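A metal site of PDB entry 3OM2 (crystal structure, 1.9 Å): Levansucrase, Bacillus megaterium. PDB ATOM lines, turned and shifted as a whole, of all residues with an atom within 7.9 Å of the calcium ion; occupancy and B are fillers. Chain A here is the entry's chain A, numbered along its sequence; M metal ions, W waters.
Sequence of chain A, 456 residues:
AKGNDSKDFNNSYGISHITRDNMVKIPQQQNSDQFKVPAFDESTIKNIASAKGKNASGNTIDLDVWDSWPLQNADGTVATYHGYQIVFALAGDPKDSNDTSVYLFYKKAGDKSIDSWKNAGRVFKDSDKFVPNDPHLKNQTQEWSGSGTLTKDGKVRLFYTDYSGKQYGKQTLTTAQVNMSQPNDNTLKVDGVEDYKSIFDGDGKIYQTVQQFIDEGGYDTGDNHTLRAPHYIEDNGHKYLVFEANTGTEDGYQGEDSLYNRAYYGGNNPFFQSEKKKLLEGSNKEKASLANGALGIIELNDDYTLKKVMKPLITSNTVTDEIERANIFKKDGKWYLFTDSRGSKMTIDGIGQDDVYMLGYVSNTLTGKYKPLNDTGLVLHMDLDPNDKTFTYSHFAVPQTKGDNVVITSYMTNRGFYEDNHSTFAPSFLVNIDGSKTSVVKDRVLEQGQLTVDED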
ATOM      1  N   GLN A 208     -20.009 -11.451   1.162  1.00  0.00           N
ATOM      2  CA  GLN A 208     -20.691 -10.410   0.399  1.00  0.00           C
ATOM      3  C   GLN A 208     -21.879 -11.001  -0.363  1.00  0.00           C
ATOM      4  O   GLN A 208     -21.784 -12.152  -0.842  1.00  0.00           O
ATOM      5  CB  GLN A 208     -19.701  -9.763  -0.592  1.00  0.00           C
ATOM      6  CG  GLN A 208     -20.224  -8.500  -1.268  1.00  0.00           C
ATOM      7  CD  GLN A 208     -19.290  -7.955  -2.308  1.00  0.00           C
ATOM      8  OE1 GLN A 208     -18.884  -8.662  -3.265  1.00  0.00           O
ATOM      9  NE2 GLN A 208     -18.964  -6.659  -2.172  1.00  0.00           N
ATOM     10  N   PHE A 213     -23.520  -5.644  -3.770  1.00  0.00           N
ATOM     11  CA  PHE A 213     -22.985  -5.236  -5.045  1.00  0.00           C
ATOM     12  C   PHE A 213     -23.899  -4.236  -5.761  1.00  0.00           C
ATOM     13  O   PHE A 213     -23.436  -3.250  -6.355  1.00  0.00           O
ATOM     14  CB  PHE A 213     -22.719  -6.488  -5.930  1.00  0.00           C
ATOM     15  CG  PHE A 213     -22.207  -6.177  -7.319  1.00  0.00           C
ATOM     16  CD1 PHE A 213     -20.957  -5.573  -7.512  1.00  0.00           C
ATOM     17  CD2 PHE A 213     -22.963  -6.520  -8.432  1.00  0.00           C
ATOM     18  CE1 PHE A 213     -20.472  -5.299  -8.794  1.00  0.00           C
ATOM     19  CE2 PHE A 213     -22.517  -6.238  -9.738  1.00  0.00           C
ATOM     20  CZ  PHE A 213     -21.262  -5.644  -9.924  1.00  0.00           C
ATOM     21  N   GLU A 216     -24.014  -0.662  -3.765  1.00  0.00           N
ATOM     22  CA  GLU A 216     -22.820   0.178  -3.896  1.00  0.00           C
ATOM     23  C   GLU A 216     -22.744   0.806  -5.275  1.00  0.00           C
ATOM     24  O   GLU A 216     -21.969   1.736  -5.483  1.00  0.00           O
ATOM     25  CB  GLU A 216     -21.539  -0.619  -3.659  1.00  0.00           C
ATOM     26  CG  GLU A 216     -21.219  -1.611  -4.788  1.00  0.00           C
ATOM     27  CD  GLU A 216     -19.989  -2.440  -4.543  1.00  0.00           C
ATOM     28  OE1 GLU A 216     -18.971  -1.881  -4.121  1.00  0.00           O
ATOM     29  OE2 GLU A 216     -20.019  -3.662  -4.829  1.00  0.00           O
ATOM     30  N   GLY A 222     -16.371  -1.084 -10.435  1.00  0.00           N
ATOM     31  CA  GLY A 222     -15.158  -1.889 -10.503  1.00  0.00           C
ATOM     32  C   GLY A 222     -15.071  -2.989  -9.460  1.00  0.00           C
ATOM     33  O   GLY A 222     -14.069  -3.654  -9.368  1.00  0.00           O
ATOM     34  N   ASP A 223     -16.127  -3.151  -8.657  1.00  0.00           N
ATOM     35  CA  ASP A 223     -16.169  -4.244  -7.691  1.00  0.00           C
ATOM     36  C   ASP A 223     -16.488  -5.506  -8.440  1.00  0.00           C
ATOM     37  O   ASP A 223     -17.127  -5.455  -9.483  1.00  0.00           O
ATOM     38  CB  ASP A 223     -17.220  -3.985  -6.613  1.00  0.00           C
ATOM     39  CG  ASP A 223     -16.980  -4.818  -5.369  1.00  0.00           C
ATOM     40  OD1 ASP A 223     -15.847  -5.333  -5.204  1.00  0.00           O
ATOM     41  OD2 ASP A 223     -17.908  -4.943  -4.561  1.00  0.00           O
ATOM     42  N   ASN A 224     -16.005  -6.630  -7.944  1.00  0.00           N
ATOM     43  CA  ASN A 224     -16.215  -7.926  -8.609  1.00  0.00           C
ATOM     44  C   ASN A 224     -16.805  -8.850  -7.553  1.00  0.00           C
ATOM     45  O   ASN A 224     -16.082  -9.346  -6.655  1.00  0.00           O
ATOM     46  CB  ASN A 224     -14.880  -8.440  -9.170  1.00  0.00           C
ATOM     47  CG  ASN A 224     -14.993  -9.782  -9.888  1.00  0.00           C
ATOM     48  OD1 ASN A 224     -16.014 -10.497  -9.840  1.00  0.00           O
ATOM     49  ND2 ASN A 224     -13.903 -10.167 -10.556  1.00  0.00           N
ATOM     50  N   HIS A 225     -18.096  -9.069  -7.647  1.00  0.00           N
ATOM     51  CA  HIS A 225     -18.799  -9.915  -6.672  1.00  0.00           C
ATOM     52  C   HIS A 225     -18.757 -11.376  -7.137  1.00  0.00           C
ATOM     53  O   HIS A 225     -19.061 -11.701  -8.307  1.00  0.00           O
ATOM     54  CB  HIS A 225     -20.261  -9.445  -6.450  1.00  0.00           C
ATOM     55  CG  HIS A 225     -21.084 -10.435  -5.703  1.00  0.00           C
ATOM     56  ND1 HIS A 225     -20.859 -10.741  -4.374  1.00  0.00           N
ATOM     57  CD2 HIS A 225     -22.058 -11.291  -6.128  1.00  0.00           C
ATOM     58  CE1 HIS A 225     -21.701 -11.701  -4.001  1.00  0.00           C
ATOM     59  NE2 HIS A 225     -22.428 -12.058  -5.048  1.00  0.00           N
ATOM     60  N   THR A 226     -18.364 -12.260  -6.222  1.00  0.00           N
ATOM     61  CA  THR A 226     -18.274 -13.690  -6.539  1.00  0.00           C
ATOM     62  C   THR A 226     -18.925 -14.551  -5.451  1.00  0.00           C
ATOM     63  O   THR A 226     -18.945 -14.163  -4.282  1.00  0.00           O
ATOM     64  CB  THR A 226     -16.831 -14.149  -6.716  1.00  0.00           C
ATOM     65  OG1 THR A 226     -16.203 -14.192  -5.442  1.00  0.00           O
ATOM     66  CG2 THR A 226     -16.020 -13.172  -7.640  1.00  0.00           C
ATOM     67  N   ALA A 245     -15.652 -16.752  -2.750  1.00  0.00           N
ATOM     68  CA  ALA A 245     -16.563 -15.662  -2.370  1.00  0.00           C
ATOM     69  C   ALA A 245     -15.765 -14.391  -2.117  1.00  0.00           C
ATOM     70  O   ALA A 245     -14.648 -14.248  -2.580  1.00  0.00           O
ATOM     71  CB  ALA A 245     -17.387 -16.049  -1.088  1.00  0.00           C
ATOM     72  N   ASN A 246     -16.395 -13.463  -1.413  1.00  0.00           N
ATOM     73  CA  ASN A 246     -15.727 -12.232  -1.000  1.00  0.00           C
ATOM     74  C   ASN A 246     -16.167 -11.967   0.445  1.00  0.00           C
ATOM     75  O   ASN A 246     -17.279 -12.378   0.855  1.00  0.00           O
ATOM     76  CB  ASN A 246     -16.112 -11.061  -1.900  1.00  0.00           C
ATOM     77  CG  ASN A 246     -15.809 -11.325  -3.371  1.00  0.00           C
ATOM     78  OD1 ASN A 246     -16.617 -11.917  -4.113  1.00  0.00           O
ATOM     79  ND2 ASN A 246     -14.649 -10.878  -3.808  1.00  0.00           N
ATOM     80  N   THR A 247     -15.324 -11.277   1.207  1.00  0.00           N
ATOM     81  CA  THR A 247     -15.689 -11.002   2.605  1.00  0.00           C
ATOM     82  C   THR A 247     -16.949 -10.155   2.719  1.00  0.00           C
ATOM     83  O   THR A 247     -17.294  -9.394   1.790  1.00  0.00           O
ATOM     84  CB  THR A 247     -14.543 -10.360   3.394  1.00  0.00           C
ATOM     85  OG1 THR A 247     -14.203  -9.078   2.812  1.00  0.00           O
ATOM     86  CG2 THR A 247     -13.331 -11.286   3.370  1.00  0.00           C
ATOM     87  N   TYR A 253     -13.963  -6.251   5.470  1.00  0.00           N
ATOM     88  CA  TYR A 253     -14.611  -5.931   4.191  1.00  0.00           C
ATOM     89  C   TYR A 253     -13.673  -5.117   3.297  1.00  0.00           C
ATOM     90  O   TYR A 253     -12.657  -4.576   3.777  1.00  0.00           O
ATOM     91  CB  TYR A 253     -15.874  -5.149   4.476  1.00  0.00           C
ATOM     92  CG  TYR A 253     -16.874  -5.086   3.331  1.00  0.00           C
ATOM     93  CD1 TYR A 253     -17.186  -6.218   2.561  1.00  0.00           C
ATOM     94  CD2 TYR A 253     -17.485  -3.886   3.012  1.00  0.00           C
ATOM     95  CE1 TYR A 253     -18.103  -6.164   1.529  1.00  0.00           C
ATOM     96  CE2 TYR A 253     -18.440  -3.804   1.929  1.00  0.00           C
ATOM     97  CZ  TYR A 253     -18.729  -4.939   1.217  1.00  0.00           C
ATOM     98  OH  TYR A 253     -19.650  -4.877   0.187  1.00  0.00           O
ATOM     99  N   GLN A 254     -14.003  -5.031   2.021  1.00  0.00           N
ATOM    100  CA  GLN A 254     -13.345  -4.089   1.116  1.00  0.00           C
ATOM    101  C   GLN A 254     -13.515  -2.669   1.668  1.00  0.00           C
ATOM    102  O   GLN A 254     -14.437  -2.383   2.469  1.00  0.00           O
ATOM    103  CB  GLN A 254     -13.980  -4.191  -0.284  1.00  0.00           C
ATOM    104  CG  GLN A 254     -15.514  -3.888  -0.279  1.00  0.00           C
ATOM    105  CD  GLN A 254     -16.173  -4.293  -1.593  1.00  0.00           C
ATOM    106  OE1 GLN A 254     -15.825  -5.317  -2.164  1.00  0.00           O
ATOM    107  NE2 GLN A 254     -17.129  -3.468  -2.087  1.00  0.00           N
ATOM    108  N   GLY A 255     -12.602  -1.791   1.267  1.00  0.00           N
ATOM    109  CA  GLY A 255     -12.657  -0.407   1.684  1.00  0.00           C
ATOM    110  C   GLY A 255     -11.286   0.174   1.802  1.00  0.00           C
ATOM    111  O   GLY A 255     -10.304  -0.578   1.907  1.00  0.00           O
ATOM    112  N   LYS A 287      -8.358  -0.546  -6.934  1.00  0.00           N
ATOM    113  CA  LYS A 287      -8.496  -1.987  -7.094  1.00  0.00           C
ATOM    114  C   LYS A 287      -8.102  -2.767  -5.814  1.00  0.00           C
ATOM    115  O   LYS A 287      -8.732  -3.775  -5.465  1.00  0.00           O
ATOM    116  CB  LYS A 287      -7.675  -2.422  -8.312  1.00  0.00           C
ATOM    117  CG  LYS A 287      -7.687  -3.873  -8.675  1.00  0.00           C
ATOM    118  CD  LYS A 287      -7.110  -3.956 -10.103  1.00  0.00           C
ATOM    119  CE  LYS A 287      -6.595  -5.321 -10.452  1.00  0.00           C
ATOM    120  NZ  LYS A 287      -5.562  -5.188 -11.518  1.00  0.00           N
ATOM    121  N   ALA A 288      -7.044  -2.308  -5.141  1.00  0.00           N
ATOM    122  CA  ALA A 288      -6.616  -2.926  -3.888  1.00  0.00           C
ATOM    123  C   ALA A 288      -7.661  -2.739  -2.797  1.00  0.00           C
ATOM    124  O   ALA A 288      -7.955  -3.683  -2.057  1.00  0.00           O
ATOM    125  CB  ALA A 288      -5.207  -2.367  -3.427  1.00  0.00           C
ATOM    126  N   SER A 289      -8.202  -1.518  -2.695  1.00  0.00           N
ATOM    127  CA  SER A 289      -9.320  -1.234  -1.790  1.00  0.00           C
ATOM    128  C   SER A 289     -10.525  -2.180  -2.003  1.00  0.00           C
ATOM    129  O   SER A 289     -11.071  -2.736  -1.050  1.00  0.00           O
ATOM    130  CB  SER A 289      -9.766   0.232  -1.920  1.00  0.00           C
ATOM    131  OG  SER A 289      -8.770   1.131  -1.477  1.00  0.00           O
ATOM    132  N   LEU A 290     -10.920  -2.344  -3.249  1.00  0.00           N
ATOM    133  CA  LEU A 290     -12.058  -3.180  -3.619  1.00  0.00           C
ATOM    134  C   LEU A 290     -11.777  -4.679  -3.499  1.00  0.00           C
ATOM    135  O   LEU A 290     -12.700  -5.486  -3.432  1.00  0.00           O
ATOM    136  CB  LEU A 290     -12.438  -2.858  -5.061  1.00  0.00           C
ATOM    137  CG  LEU A 290     -13.231  -1.547  -5.272  1.00  0.00           C
ATOM    138  CD1 LEU A 290     -13.355  -1.329  -6.747  1.00  0.00           C
ATOM    139  CD2 LEU A 290     -14.573  -1.608  -4.599  1.00  0.00           C
ATOM    140  N   ALA A 291     -10.508  -5.064  -3.463  1.00  0.00           N
ATOM    141  CA  ALA A 291     -10.106  -6.469  -3.458  1.00  0.00           C
ATOM    142  C   ALA A 291     -10.359  -7.131  -2.108  1.00  0.00           C
ATOM    143  O   ALA A 291      -9.661  -6.840  -1.135  1.00  0.00           O
ATOM    144  CB  ALA A 291      -8.625  -6.602  -3.851  1.00  0.00           C
ATOM    145  N   ASN A 292     -11.348  -8.021  -2.053  1.00  0.00           N
ATOM    146  CA  ASN A 292     -11.638  -8.774  -0.825  1.00  0.00           C
ATOM    147  C   ASN A 292     -12.058 -10.243  -1.084  1.00  0.00           C
ATOM    148  O   ASN A 292     -13.009 -10.759  -0.490  1.00  0.00           O
ATOM    149  CB  ASN A 292     -12.645  -7.998   0.050  1.00  0.00           C
ATOM    150  CG  ASN A 292     -14.022  -7.964  -0.573  1.00  0.00           C
ATOM    151  OD1 ASN A 292     -14.158  -7.978  -1.781  1.00  0.00           O
ATOM    152  ND2 ASN A 292     -15.041  -7.932   0.251  1.00  0.00           N
ATOM    153  N   GLY A 293     -11.314 -10.919  -1.968  1.00  0.00           N
ATOM    154  CA  GLY A 293     -11.624 -12.295  -2.321  1.00  0.00           C
ATOM    155  C   GLY A 293     -11.503 -13.179  -1.097  1.00  0.00           C
ATOM    156  O   GLY A 293     -10.761 -12.843  -0.149  1.00  0.00           O
ATOM    157  N   ASN A 317      -7.525 -10.041   0.752  1.00  0.00           N
ATOM    158  CA  ASN A 317      -7.818  -8.610   0.875  1.00  0.00           C
ATOM    159  C   ASN A 317      -6.617  -7.826   0.348  1.00  0.00           C
ATOM    160  O   ASN A 317      -5.464  -8.180   0.652  1.00  0.00           O
ATOM    161  CB  ASN A 317      -8.105  -8.211   2.325  1.00  0.00           C
ATOM    162  CG  ASN A 317      -9.504  -8.524   2.769  1.00  0.00           C
ATOM    163  OD1 ASN A 317     -10.412  -7.663   2.723  1.00  0.00           O
ATOM    164  ND2 ASN A 317      -9.714  -9.743   3.197  1.00  0.00           N
ATOM    165  N   THR A 320      -6.399  -9.329  -4.549  1.00  0.00           N
ATOM    166  CA  THR A 320      -7.325  -9.557  -5.657  1.00  0.00           C
ATOM    167  C   THR A 320      -8.757  -9.756  -5.141  1.00  0.00           C
ATOM    168  O   THR A 320      -8.976 -10.146  -3.990  1.00  0.00           O
ATOM    169  CB  THR A 320      -6.904 -10.756  -6.536  1.00  0.00           C
ATOM    170  OG1 THR A 320      -7.862 -10.933  -7.598  1.00  0.00           O
ATOM    171  CG2 THR A 320      -6.755 -12.076  -5.718  1.00  0.00           C
ATOM    172  N   ASP A 321      -9.725  -9.478  -6.022  1.00  0.00           N
ATOM    173  CA  ASP A 321     -11.115  -9.781  -5.752  1.00  0.00           C
ATOM    174  C   ASP A 321     -11.492 -11.195  -6.190  1.00  0.00           C
ATOM    175  O   ASP A 321     -12.641 -11.633  -5.999  1.00  0.00           O
ATOM    176  CB  ASP A 321     -12.031  -8.777  -6.446  1.00  0.00           C
ATOM    177  CG  ASP A 321     -12.997  -8.099  -5.485  1.00  0.00           C
ATOM    178  OD1 ASP A 321     -12.976  -8.428  -4.273  1.00  0.00           O
ATOM    179  OD2 ASP A 321     -13.748  -7.213  -5.905  1.00  0.00           O
ATOM    180  N   GLU A 322     -10.536 -11.912  -6.807  1.00  0.00           N
ATOM    181  CA  GLU A 322     -10.875 -13.140  -7.546  1.00  0.00           C
ATOM    182  C   GLU A 322      -9.882 -14.279  -7.286  1.00  0.00           C
ATOM    183  O   GLU A 322      -8.838 -14.363  -7.929  1.00  0.00           O
ATOM    184  CB  GLU A 322     -10.937 -12.868  -9.046  1.00  0.00           C
ATOM    185  CG  GLU A 322     -12.296 -12.528  -9.537  1.00  0.00           C
ATOM    186  CD  GLU A 322     -12.537 -12.971 -10.990  1.00  0.00           C
ATOM    187  OE1 GLU A 322     -11.554 -13.206 -11.765  1.00  0.00           O
ATOM    188  OE2 GLU A 322     -13.713 -13.077 -11.359  1.00  0.00           O
HETATM  189 CA    CA M   1     -14.746  -6.651  -3.706  1.00  0.00          CA
HETATM  190  O   HOH W   1     -16.525  -8.299  -4.084  1.00  0.00           O
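Within 4 Å of the calcium ion: Asp 223, Gln 254, Leu 290, Asn 292 and Asp 321.
The calcium ion is bound by OD1 of Asp 223 (2.3 Å), OE1 of Gln 254 (2.3 Å), O of Leu 290 (2.4 Å), OD1 of Asn 292 (2.4 Å), water W1 (2.5 Å), OD2 of Asp 321 (2.5 Å) and OD1 of Asp 321 (2.6 Å). The calcium ion has seven donor atoms within binding distance.
Water W1 lies within hydrogen-bond range of the side-chain amide oxygen (OE1) of Gln 208 (2.5 Å), the backbone carbonyl oxygen (O) of Asn 224 (2.8 Å) and the side-chain amide nitrogen (ND2) of Asn 246 (3.2 Å).
The side-chain carboxylate (OD2) of Asp 223 lies within hydrogen-bond range of the side-chain amide nitrogen (NE2) of Gln 208 (3.1 Å). OD2 of Asp 223 lies close to OE2 of Glu 216. The side-chain amide nitrogen (NE2) of Gln 208 lies close to the side-chain amide oxygen (OE1) of Gln 254. NE2 of Gln 254 is in hydrogen-bond range of OE1 of Glu 216, 3.2 Å away. O of Asn 292 lies within hydrogen-bond range of N of Thr 247, at 2.9 Å. OD2 of Asp 321 sits close to N of Asn 224 (3.1 Å). O of Asp 321 is in hydrogen-bond range of ND2 of Asn 246 (3.1 Å).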
